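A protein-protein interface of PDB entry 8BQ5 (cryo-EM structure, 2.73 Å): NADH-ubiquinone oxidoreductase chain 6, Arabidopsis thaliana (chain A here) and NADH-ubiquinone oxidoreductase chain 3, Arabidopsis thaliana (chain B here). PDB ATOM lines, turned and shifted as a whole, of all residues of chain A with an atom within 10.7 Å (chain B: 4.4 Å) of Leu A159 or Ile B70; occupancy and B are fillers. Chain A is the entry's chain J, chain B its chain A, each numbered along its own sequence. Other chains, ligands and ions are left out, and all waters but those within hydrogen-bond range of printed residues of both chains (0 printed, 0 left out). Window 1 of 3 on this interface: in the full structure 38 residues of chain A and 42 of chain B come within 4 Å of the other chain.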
ATOM      1  N   VAL A  55      22.370  -0.479 -15.449  1.00  0.00           N
ATOM      2  CA  VAL A  55      21.180   0.353 -15.290  1.00  0.00           C
ATOM      3  C   VAL A  55      21.319   1.653 -16.075  1.00  0.00           C
ATOM      4  O   VAL A  55      20.382   2.086 -16.755  1.00  0.00           O
ATOM      5  CB  VAL A  55      20.914   0.614 -13.795  1.00  0.00           C
ATOM      6  CG1 VAL A  55      19.931   1.758 -13.612  1.00  0.00           C
ATOM      7  CG2 VAL A  55      20.401  -0.647 -13.123  1.00  0.00           C
ATOM      8  N   VAL A  56      22.486   2.286 -16.008  1.00  0.00           N
ATOM      9  CA  VAL A  56      22.655   3.623 -16.563  1.00  0.00           C
ATOM     10  C   VAL A  56      23.206   3.577 -17.983  1.00  0.00           C
ATOM     11  O   VAL A  56      22.619   4.153 -18.902  1.00  0.00           O
ATOM     12  CB  VAL A  56      23.556   4.467 -15.635  1.00  0.00           C
ATOM     13  CG1 VAL A  56      23.877   5.802 -16.281  1.00  0.00           C
ATOM     14  CG2 VAL A  56      22.886   4.666 -14.287  1.00  0.00           C
ATOM     15  N   GLY A  59      20.870   0.716 -19.817  1.00  0.00           N
ATOM     16  CA  GLY A  59      19.446   0.927 -19.637  1.00  0.00           C
ATOM     17  C   GLY A  59      18.975   2.312 -20.028  1.00  0.00           C
ATOM     18  O   GLY A  59      17.820   2.484 -20.427  1.00  0.00           O
ATOM     19  N   ALA A  60      19.843   3.317 -19.915  1.00  0.00           N
ATOM     20  CA  ALA A  60      19.447   4.692 -20.190  1.00  0.00           C
ATOM     21  C   ALA A  60      20.219   5.326 -21.336  1.00  0.00           C
ATOM     22  O   ALA A  60      19.603   5.824 -22.285  1.00  0.00           O
ATOM     23  CB  ALA A  60      19.603   5.543 -18.920  1.00  0.00           C
ATOM     24  N   ILE A  61      21.552   5.324 -21.278  1.00  0.00           N
ATOM     25  CA  ILE A  61      22.349   6.053 -22.261  1.00  0.00           C
ATOM     26  C   ILE A  61      22.298   5.363 -23.620  1.00  0.00           C
ATOM     27  O   ILE A  61      22.049   6.000 -24.655  1.00  0.00           O
ATOM     28  CB  ILE A  61      23.797   6.212 -21.760  1.00  0.00           C
ATOM     29  CG1 ILE A  61      23.834   7.133 -20.537  1.00  0.00           C
ATOM     30  CG2 ILE A  61      24.702   6.726 -22.868  1.00  0.00           C
ATOM     31  CD1 ILE A  61      25.181   7.209 -19.851  1.00  0.00           C
ATOM     32  N   LEU A  64      19.046   5.831 -25.300  1.00  0.00           N
ATOM     33  CA  LEU A  64      19.008   7.149 -25.927  1.00  0.00           C
ATOM     34  C   LEU A  64      19.691   7.129 -27.290  1.00  0.00           C
ATOM     35  O   LEU A  64      19.134   7.601 -28.293  1.00  0.00           O
ATOM     36  CB  LEU A  64      19.674   8.165 -24.998  1.00  0.00           C
ATOM     37  CG  LEU A  64      19.843   9.620 -25.431  1.00  0.00           C
ATOM     38  CD1 LEU A  64      18.524  10.256 -25.811  1.00  0.00           C
ATOM     39  CD2 LEU A  64      20.549  10.418 -24.341  1.00  0.00           C
ATOM     40  N   TRP A 151      29.857  17.993  -3.953  1.00  0.00           N
ATOM     41  CA  TRP A 151      30.031  17.410  -5.282  1.00  0.00           C
ATOM     42  C   TRP A 151      28.747  16.740  -5.766  1.00  0.00           C
ATOM     43  O   TRP A 151      28.401  16.813  -6.952  1.00  0.00           O
ATOM     44  CB  TRP A 151      31.197  16.419  -5.263  1.00  0.00           C
ATOM     45  CG  TRP A 151      32.495  16.996  -4.743  1.00  0.00           C
ATOM     46  CD1 TRP A 151      32.809  18.318  -4.605  1.00  0.00           C
ATOM     47  CD2 TRP A 151      33.656  16.266  -4.327  1.00  0.00           C
ATOM     48  NE1 TRP A 151      34.084  18.455  -4.117  1.00  0.00           N
ATOM     49  CE2 TRP A 151      34.627  17.210  -3.939  1.00  0.00           C
ATOM     50  CE3 TRP A 151      33.964  14.906  -4.236  1.00  0.00           C
ATOM     51  CZ2 TRP A 151      35.884  16.837  -3.472  1.00  0.00           C
ATOM     52  CZ3 TRP A 151      35.215  14.539  -3.778  1.00  0.00           C
ATOM     53  CH2 TRP A 151      36.158  15.500  -3.397  1.00  0.00           C
ATOM     54  N   PHE A 152      28.028  16.090  -4.850  1.00  0.00           N
ATOM     55  CA  PHE A 152      26.717  15.514  -5.131  1.00  0.00           C
ATOM     56  C   PHE A 152      25.749  16.571  -5.671  1.00  0.00           C
ATOM     57  O   PHE A 152      25.102  16.386  -6.717  1.00  0.00           O
ATOM     58  CB  PHE A 152      26.215  14.881  -3.826  1.00  0.00           C
ATOM     59  CG  PHE A 152      24.845  14.281  -3.887  1.00  0.00           C
ATOM     60  CD1 PHE A 152      24.511  13.347  -4.849  1.00  0.00           C
ATOM     61  CD2 PHE A 152      23.906  14.604  -2.919  1.00  0.00           C
ATOM     62  CE1 PHE A 152      23.250  12.783  -4.870  1.00  0.00           C
ATOM     63  CE2 PHE A 152      22.651  14.045  -2.936  1.00  0.00           C
ATOM     64  CZ  PHE A 152      22.322  13.132  -3.911  1.00  0.00           C
ATOM     65  N   LEU A 153      25.672  17.713  -4.986  1.00  0.00           N
ATOM     66  CA  LEU A 153      24.757  18.766  -5.416  1.00  0.00           C
ATOM     67  C   LEU A 153      25.202  19.399  -6.735  1.00  0.00           C
ATOM     68  O   LEU A 153      24.364  19.780  -7.564  1.00  0.00           O
ATOM     69  CB  LEU A 153      24.628  19.813  -4.313  1.00  0.00           C
ATOM     70  CG  LEU A 153      24.030  19.268  -3.014  1.00  0.00           C
ATOM     71  CD1 LEU A 153      23.848  20.371  -1.991  1.00  0.00           C
ATOM     72  CD2 LEU A 153      22.710  18.562  -3.286  1.00  0.00           C
ATOM     73  N   VAL A 154      26.513  19.517  -6.956  1.00  0.00           N
ATOM     74  CA  VAL A 154      26.989  20.049  -8.233  1.00  0.00           C
ATOM     75  C   VAL A 154      26.620  19.106  -9.374  1.00  0.00           C
ATOM     76  O   VAL A 154      26.278  19.546 -10.481  1.00  0.00           O
ATOM     77  CB  VAL A 154      28.505  20.318  -8.178  1.00  0.00           C
ATOM     78  CG1 VAL A 154      29.030  20.684  -9.557  1.00  0.00           C
ATOM     79  CG2 VAL A 154      28.806  21.433  -7.194  1.00  0.00           C
ATOM     80  N   SER A 155      26.674  17.795  -9.124  1.00  0.00           N
ATOM     81  CA  SER A 155      26.219  16.838 -10.129  1.00  0.00           C
ATOM     82  C   SER A 155      24.733  17.023 -10.429  1.00  0.00           C
ATOM     83  O   SER A 155      24.299  16.911 -11.587  1.00  0.00           O
ATOM     84  CB  SER A 155      26.505  15.412  -9.661  1.00  0.00           C
ATOM     85  OG  SER A 155      25.437  14.912  -8.875  1.00  0.00           O
ATOM     86  N   SER A 156      23.938  17.313  -9.397  1.00  0.00           N
ATOM     87  CA  SER A 156      22.532  17.642  -9.638  1.00  0.00           C
ATOM     88  C   SER A 156      22.390  18.876 -10.529  1.00  0.00           C
ATOM     89  O   SER A 156      21.518  18.923 -11.408  1.00  0.00           O
ATOM     90  CB  SER A 156      21.801  17.864  -8.317  1.00  0.00           C
ATOM     91  OG  SER A 156      21.995  19.179  -7.839  1.00  0.00           O
ATOM     92  N   LEU A 157      23.221  19.894 -10.298  1.00  0.00           N
ATOM     93  CA  LEU A 157      23.184  21.084 -11.150  1.00  0.00           C
ATOM     94  C   LEU A 157      23.501  20.733 -12.599  1.00  0.00           C
ATOM     95  O   LEU A 157      22.882  21.262 -13.536  1.00  0.00           O
ATOM     96  CB  LEU A 157      24.162  22.134 -10.627  1.00  0.00           C
ATOM     97  CG  LEU A 157      23.708  22.931  -9.406  1.00  0.00           C
ATOM     98  CD1 LEU A 157      24.698  24.043  -9.103  1.00  0.00           C
ATOM     99  CD2 LEU A 157      22.313  23.490  -9.634  1.00  0.00           C
ATOM    100  N   ILE A 158      24.468  19.837 -12.798  1.00  0.00           N
ATOM    101  CA  ILE A 158      24.804  19.364 -14.139  1.00  0.00           C
ATOM    102  C   ILE A 158      23.589  18.714 -14.801  1.00  0.00           C
ATOM    103  O   ILE A 158      23.274  18.978 -15.973  1.00  0.00           O
ATOM    104  CB  ILE A 158      26.006  18.400 -14.057  1.00  0.00           C
ATOM    105  CG1 ILE A 158      27.289  19.176 -13.744  1.00  0.00           C
ATOM    106  CG2 ILE A 158      26.154  17.594 -15.324  1.00  0.00           C
ATOM    107  CD1 ILE A 158      28.445  18.303 -13.297  1.00  0.00           C
ATOM    108  N   LEU A 159      22.874  17.870 -14.053  1.00  0.00           N
ATOM    109  CA  LEU A 159      21.693  17.214 -14.615  1.00  0.00           C
ATOM    110  C   LEU A 159      20.601  18.224 -14.968  1.00  0.00           C
ATOM    111  O   LEU A 159      19.921  18.086 -15.997  1.00  0.00           O
ATOM    112  CB  LEU A 159      21.163  16.165 -13.641  1.00  0.00           C
ATOM    113  CG  LEU A 159      22.083  14.958 -13.457  1.00  0.00           C
ATOM    114  CD1 LEU A 159      21.471  13.967 -12.487  1.00  0.00           C
ATOM    115  CD2 LEU A 159      22.383  14.301 -14.797  1.00  0.00           C
ATOM    116  N   LEU A 160      20.410  19.236 -14.120  1.00  0.00           N
ATOM    117  CA  LEU A 160      19.419  20.268 -14.416  1.00  0.00           C
ATOM    118  C   LEU A 160      19.763  21.006 -15.705  1.00  0.00           C
ATOM    119  O   LEU A 160      18.876  21.308 -16.521  1.00  0.00           O
ATOM    120  CB  LEU A 160      19.317  21.249 -13.248  1.00  0.00           C
ATOM    121  CG  LEU A 160      18.540  22.537 -13.520  1.00  0.00           C
ATOM    122  CD1 LEU A 160      17.075  22.227 -13.710  1.00  0.00           C
ATOM    123  CD2 LEU A 160      18.732  23.546 -12.398  1.00  0.00           C
ATOM    124  N   VAL A 161      21.049  21.314 -15.899  1.00  0.00           N
ATOM    125  CA  VAL A 161      21.481  21.926 -17.154  1.00  0.00           C
ATOM    126  C   VAL A 161      21.132  21.022 -18.328  1.00  0.00           C
ATOM    127  O   VAL A 161      20.677  21.494 -19.378  1.00  0.00           O
ATOM    128  CB  VAL A 161      22.987  22.242 -17.113  1.00  0.00           C
ATOM    129  CG1 VAL A 161      23.487  22.617 -18.497  1.00  0.00           C
ATOM    130  CG2 VAL A 161      23.261  23.369 -16.136  1.00  0.00           C
ATOM    131  N   ALA A 162      21.343  19.713 -18.172  1.00  0.00           N
ATOM    132  CA  ALA A 162      21.004  18.785 -19.249  1.00  0.00           C
ATOM    133  C   ALA A 162      19.523  18.875 -19.613  1.00  0.00           C
ATOM    134  O   ALA A 162      19.165  18.944 -20.796  1.00  0.00           O
ATOM    135  CB  ALA A 162      21.373  17.355 -18.853  1.00  0.00           C
ATOM    136  N   MET A 163      18.646  18.880 -18.604  1.00  0.00           N
ATOM    137  CA  MET A 163      17.208  18.951 -18.876  1.00  0.00           C
ATOM    138  C   MET A 163      16.842  20.240 -19.610  1.00  0.00           C
ATOM    139  O   MET A 163      16.139  20.219 -20.637  1.00  0.00           O
ATOM    140  CB  MET A 163      16.410  18.838 -17.575  1.00  0.00           C
ATOM    141  CG  MET A 163      16.948  17.815 -16.596  1.00  0.00           C
ATOM    142  SD  MET A 163      16.157  17.866 -14.976  1.00  0.00           S
ATOM    143  CE  MET A 163      14.496  17.354 -15.392  1.00  0.00           C
ATOM    144  N   ILE A 164      17.323  21.377 -19.099  1.00  0.00           N
ATOM    145  CA  ILE A 164      16.983  22.661 -19.709  1.00  0.00           C
ATOM    146  C   ILE A 164      17.482  22.718 -21.147  1.00  0.00           C
ATOM    147  O   ILE A 164      16.768  23.169 -22.051  1.00  0.00           O
ATOM    148  CB  ILE A 164      17.544  23.826 -18.874  1.00  0.00           C
ATOM    149  CG1 ILE A 164      16.744  23.995 -17.586  1.00  0.00           C
ATOM    150  CG2 ILE A 164      17.531  25.114 -19.683  1.00  0.00           C
ATOM    151  CD1 ILE A 164      17.423  24.873 -16.571  1.00  0.00           C
ATOM    152  N   GLY A 165      18.723  22.282 -21.375  1.00  0.00           N
ATOM    153  CA  GLY A 165      19.271  22.319 -22.719  1.00  0.00           C
ATOM    154  C   GLY A 165      18.505  21.436 -23.680  1.00  0.00           C
ATOM    155  O   GLY A 165      18.215  21.837 -24.813  1.00  0.00           O
ATOM    156  N   ALA A 166      18.145  20.230 -23.235  1.00  0.00           N
ATOM    157  CA  ALA A 166      17.353  19.344 -24.075  1.00  0.00           C
ATOM    158  C   ALA A 166      16.056  20.014 -24.502  1.00  0.00           C
ATOM    159  O   ALA A 166      15.665  19.931 -25.671  1.00  0.00           O
ATOM    160  CB  ALA A 166      17.062  18.037 -23.340  1.00  0.00           C
ATOM    161  N   ILE A 167      15.383  20.700 -23.576  1.00  0.00           N
ATOM    162  CA  ILE A 167      14.132  21.357 -23.951  1.00  0.00           C
ATOM    163  C   ILE A 167      14.387  22.520 -24.902  1.00  0.00           C
ATOM    164  O   ILE A 167      13.771  22.611 -25.969  1.00  0.00           O
ATOM    165  CB  ILE A 167      13.358  21.817 -22.708  1.00  0.00           C
ATOM    166  CG1 ILE A 167      12.746  20.617 -22.015  1.00  0.00           C
ATOM    167  CG2 ILE A 167      12.273  22.806 -23.100  1.00  0.00           C
ATOM    168  CD1 ILE A 167      12.076  19.629 -22.936  1.00  0.00           C
ATOM    169  N   ILE B  66      15.481  11.367 -22.562  1.00  0.00           N
ATOM    170  CA  ILE B  66      16.180  12.300 -21.677  1.00  0.00           C
ATOM    171  C   ILE B  66      15.598  12.237 -20.269  1.00  0.00           C
ATOM    172  O   ILE B  66      16.331  12.147 -19.272  1.00  0.00           O
ATOM    173  CB  ILE B  66      16.109  13.730 -22.245  1.00  0.00           C
ATOM    174  CG1 ILE B  66      16.871  13.829 -23.562  1.00  0.00           C
ATOM    175  CG2 ILE B  66      16.665  14.730 -21.248  1.00  0.00           C
ATOM    176  CD1 ILE B  66      18.193  13.138 -23.542  1.00  0.00           C
ATOM    177  N   LEU B  67      14.268  12.299 -20.169  1.00  0.00           N
ATOM    178  CA  LEU B  67      13.635  12.241 -18.854  1.00  0.00           C
ATOM    179  C   LEU B  67      13.909  10.915 -18.163  1.00  0.00           C
ATOM    180  O   LEU B  67      14.145  10.873 -16.946  1.00  0.00           O
ATOM    181  CB  LEU B  67      12.130  12.473 -18.956  1.00  0.00           C
ATOM    182  CG  LEU B  67      11.682  13.928 -19.038  1.00  0.00           C
ATOM    183  CD1 LEU B  67      11.335  14.342 -20.444  1.00  0.00           C
ATOM    184  CD2 LEU B  67      10.531  14.163 -18.094  1.00  0.00           C
ATOM    185  N   PHE B  68      13.867   9.816 -18.918  1.00  0.00           N
ATOM    186  CA  PHE B  68      14.181   8.526 -18.326  1.00  0.00           C
ATOM    187  C   PHE B  68      15.606   8.500 -17.802  1.00  0.00           C
ATOM    188  O   PHE B  68      15.867   7.941 -16.737  1.00  0.00           O
ATOM    189  CB  PHE B  68      13.984   7.401 -19.333  1.00  0.00           C
ATOM    190  CG  PHE B  68      14.320   6.059 -18.776  1.00  0.00           C
ATOM    191  CD1 PHE B  68      13.678   5.597 -17.642  1.00  0.00           C
ATOM    192  CD2 PHE B  68      15.306   5.279 -19.346  1.00  0.00           C
ATOM    193  CE1 PHE B  68      13.986   4.372 -17.106  1.00  0.00           C
ATOM    194  CE2 PHE B  68      15.622   4.049 -18.812  1.00  0.00           C
ATOM    195  CZ  PHE B  68      14.961   3.595 -17.691  1.00  0.00           C
ATOM    196  N   LEU B  69      16.545   9.080 -18.550  1.00  0.00           N
ATOM    197  CA  LEU B  69      17.937   9.091 -18.116  1.00  0.00           C
ATOM    198  C   LEU B  69      18.093   9.859 -16.807  1.00  0.00           C
ATOM    199  O   LEU B  69      18.765   9.397 -15.872  1.00  0.00           O
ATOM    200  CB  LEU B  69      18.801   9.699 -19.222  1.00  0.00           C
ATOM    201  CG  LEU B  69      20.238  10.096 -18.900  1.00  0.00           C
ATOM    202  CD1 LEU B  69      21.088   8.853 -18.717  1.00  0.00           C
ATOM    203  CD2 LEU B  69      20.789  10.987 -19.999  1.00  0.00           C
ATOM    204  N   ILE B  70      17.443  11.022 -16.714  1.00  0.00           N
ATOM    205  CA  ILE B  70      17.525  11.826 -15.495  1.00  0.00           C
ATOM    206  C   ILE B  70      16.968  11.053 -14.301  1.00  0.00           C
ATOM    207  O   ILE B  70      17.614  10.940 -13.249  1.00  0.00           O
ATOM    208  CB  ILE B  70      16.794  13.169 -15.684  1.00  0.00           C
ATOM    209  CG1 ILE B  70      17.472  14.017 -16.766  1.00  0.00           C
ATOM    210  CG2 ILE B  70      16.701  13.919 -14.361  1.00  0.00           C
ATOM    211  CD1 ILE B  70      18.982  14.048 -16.682  1.00  0.00           C
ATOM    212  N   PHE B  71      15.766  10.493 -14.444  1.00  0.00           N
ATOM    213  CA  PHE B  71      15.172   9.820 -13.292  1.00  0.00           C
ATOM    214  C   PHE B  71      15.833   8.480 -12.990  1.00  0.00           C
ATOM    215  O   PHE B  71      15.805   8.029 -11.838  1.00  0.00           O
ATOM    216  CB  PHE B  71      13.670   9.664 -13.495  1.00  0.00           C
ATOM    217  CG  PHE B  71      12.901  10.899 -13.151  1.00  0.00           C
ATOM    218  CD1 PHE B  71      12.699  11.889 -14.095  1.00  0.00           C
ATOM    219  CD2 PHE B  71      12.420  11.091 -11.869  1.00  0.00           C
ATOM    220  CE1 PHE B  71      12.005  13.036 -13.774  1.00  0.00           C
ATOM    221  CE2 PHE B  71      11.728  12.236 -11.542  1.00  0.00           C
ATOM    222  CZ  PHE B  71      11.519  13.210 -12.497  1.00  0.00           C
ATOM    223  N   ASP B  72      16.457   7.852 -13.985  1.00  0.00           N
ATOM    224  CA  ASP B  72      17.257   6.662 -13.736  1.00  0.00           C
ATOM    225  C   ASP B  72      18.466   6.995 -12.873  1.00  0.00           C
ATOM    226  O   ASP B  72      18.799   6.258 -11.937  1.00  0.00           O
ATOM    227  CB  ASP B  72      17.685   6.053 -15.069  1.00  0.00           C
ATOM    228  CG  ASP B  72      17.949   4.577 -14.972  1.00  0.00           C
ATOM    229  OD1 ASP B  72      18.994   4.137 -15.489  1.00  0.00           O
ATOM    230  OD2 ASP B  72      17.119   3.859 -14.377  1.00  0.00           O
ATOM    231  N   LEU B  73      19.134   8.115 -13.167  1.00  0.00           N
ATOM    232  CA  LEU B  73      20.204   8.558 -12.277  1.00  0.00           C
ATOM    233  C   LEU B  73      19.676   8.902 -10.890  1.00  0.00           C
ATOM    234  O   LEU B  73      20.378   8.702  -9.891  1.00  0.00           O
ATOM    235  CB  LEU B  73      20.936   9.759 -12.863  1.00  0.00           C
ATOM    236  CG  LEU B  73      21.905   9.445 -13.997  1.00  0.00           C
ATOM    237  CD1 LEU B  73      21.877  10.568 -15.005  1.00  0.00           C
ATOM    238  CD2 LEU B  73      23.308   9.215 -13.454  1.00  0.00           C
ATOM    239  N   GLU B  74      18.452   9.412 -10.788  1.00  0.00           N
ATOM    240  CA  GLU B  74      17.862   9.718  -9.453  1.00  0.00           C
ATOM    241  C   GLU B  74      17.702   8.419  -8.657  1.00  0.00           C
ATOM    242  O   GLU B  74      18.134   8.398  -7.499  1.00  0.00           O
ATOM    243  CB  GLU B  74      16.559  10.501  -9.614  1.00  0.00           C
ATOM    244  CG  GLU B  74      16.024  11.104  -8.335  1.00  0.00           C
ATOM    245  CD  GLU B  74      14.779  11.946  -8.554  1.00  0.00           C
ATOM    246  OE1 GLU B  74      13.675  11.373  -8.566  1.00  0.00           O
ATOM    247  OE2 GLU B  74      14.920  13.173  -8.724  1.00  0.00           O
ATOM    248  N   LEU B 103      16.392  18.700  -8.894  1.00  0.00           N
ATOM    249  CA  LEU B 103      15.861  17.893  -9.991  1.00  0.00           C
ATOM    250  C   LEU B 103      14.357  18.096 -10.179  1.00  0.00           C
ATOM    251  O   LEU B 103      13.854  17.986 -11.301  1.00  0.00           O
ATOM    252  CB  LEU B 103      16.197  16.419  -9.767  1.00  0.00           C
ATOM    253  CG  LEU B 103      17.687  16.077  -9.897  1.00  0.00           C
ATOM    254  CD1 LEU B 103      17.885  14.593 -10.142  1.00  0.00           C
ATOM    255  CD2 LEU B 103      18.350  16.891 -11.005  1.00  0.00           C
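Val A56 touches Asp B72. Gly A59 touches Phe B68 (O to CE2, 3.1 Å). CB of Ala A60 touches CD1 of Leu B69 (3.6 Å). Asp B72 touches Ala A60 (OD1 to CB, 3.8 Å). Ile A61 touches Leu B69 (CG1 to CD1, 3.7 Å). Ile B66 touches Leu A64 (CD1 to CD1, 3.7 Å). Leu B103 touches Ser A156. Leu A159 touches Ile B70. CB of Leu A159 touches CD2 of Leu B103, 3.9 Å away. Ile B66 touches Ala A166 (CG2 to CB, 3.9 Å).
Of chain B, only Ile B70 (3.9 Å), Leu B73 (3.8 Å) and Leu B103 (3.9 Å) come within 4 Å of Leu A159. Ile B70 touches just these residues of chain A: Leu A159 and Met A163. Of the printed residues of chain A, Leu B69 touches Ala A60 (3.6 Å) and Ile A61 (3.7 Å). Phe B71 touches none of the printed residues of chain A. Printed residues of chain B within 4 Å of Ala A166: Ile B66. Of the printed residues of chain A, Ile B66 touches Leu A64 and Ala A166. Val A154 touches none of the printed residues of chain B. Gly A165 touches none of the printed residues of chain B.
O of Val A55 is in hydrogen-bond range of N of Ala A60, 3.4 Å away. The backbone carbonyl oxygen (O) of Val A56 lies within hydrogen-bond range of the backbone NH (N) of Ile A61, at 2.9 Å. The backbone carbonyl oxygen (O) of Leu A153 lies within hydrogen-bond range of the side-chain hydroxyl (OG) of Ser A156, at 2.5 Å.
The backbone carbonyl oxygen (O) of Val A55 lies close to the side-chain carboxylate (OD1) of Asp B72, at 2.8 Å.
Of the 23 printed residues of chain A, 10 touch a printed residue of chain B. Hydrophobic or aromatic side chains of chain A that line the printed part of chain B: Val A55, Ala A60, Ile A61, Leu A64, Leu A159, Met A163 and Ala A166. Of the 10 printed residues of chain B, 7 touch a printed residue of chain A. Hydrophobic or aromatic side chains of chain B that line the printed part of chain A: Ile B66, Phe B68, Leu B69, Ile B70, Leu B73 and Leu B103. Among the printed residues, no Asp or Glu carboxylate lies within 4 Å of a Lys or Arg side-chain nitrogen of the other chain.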
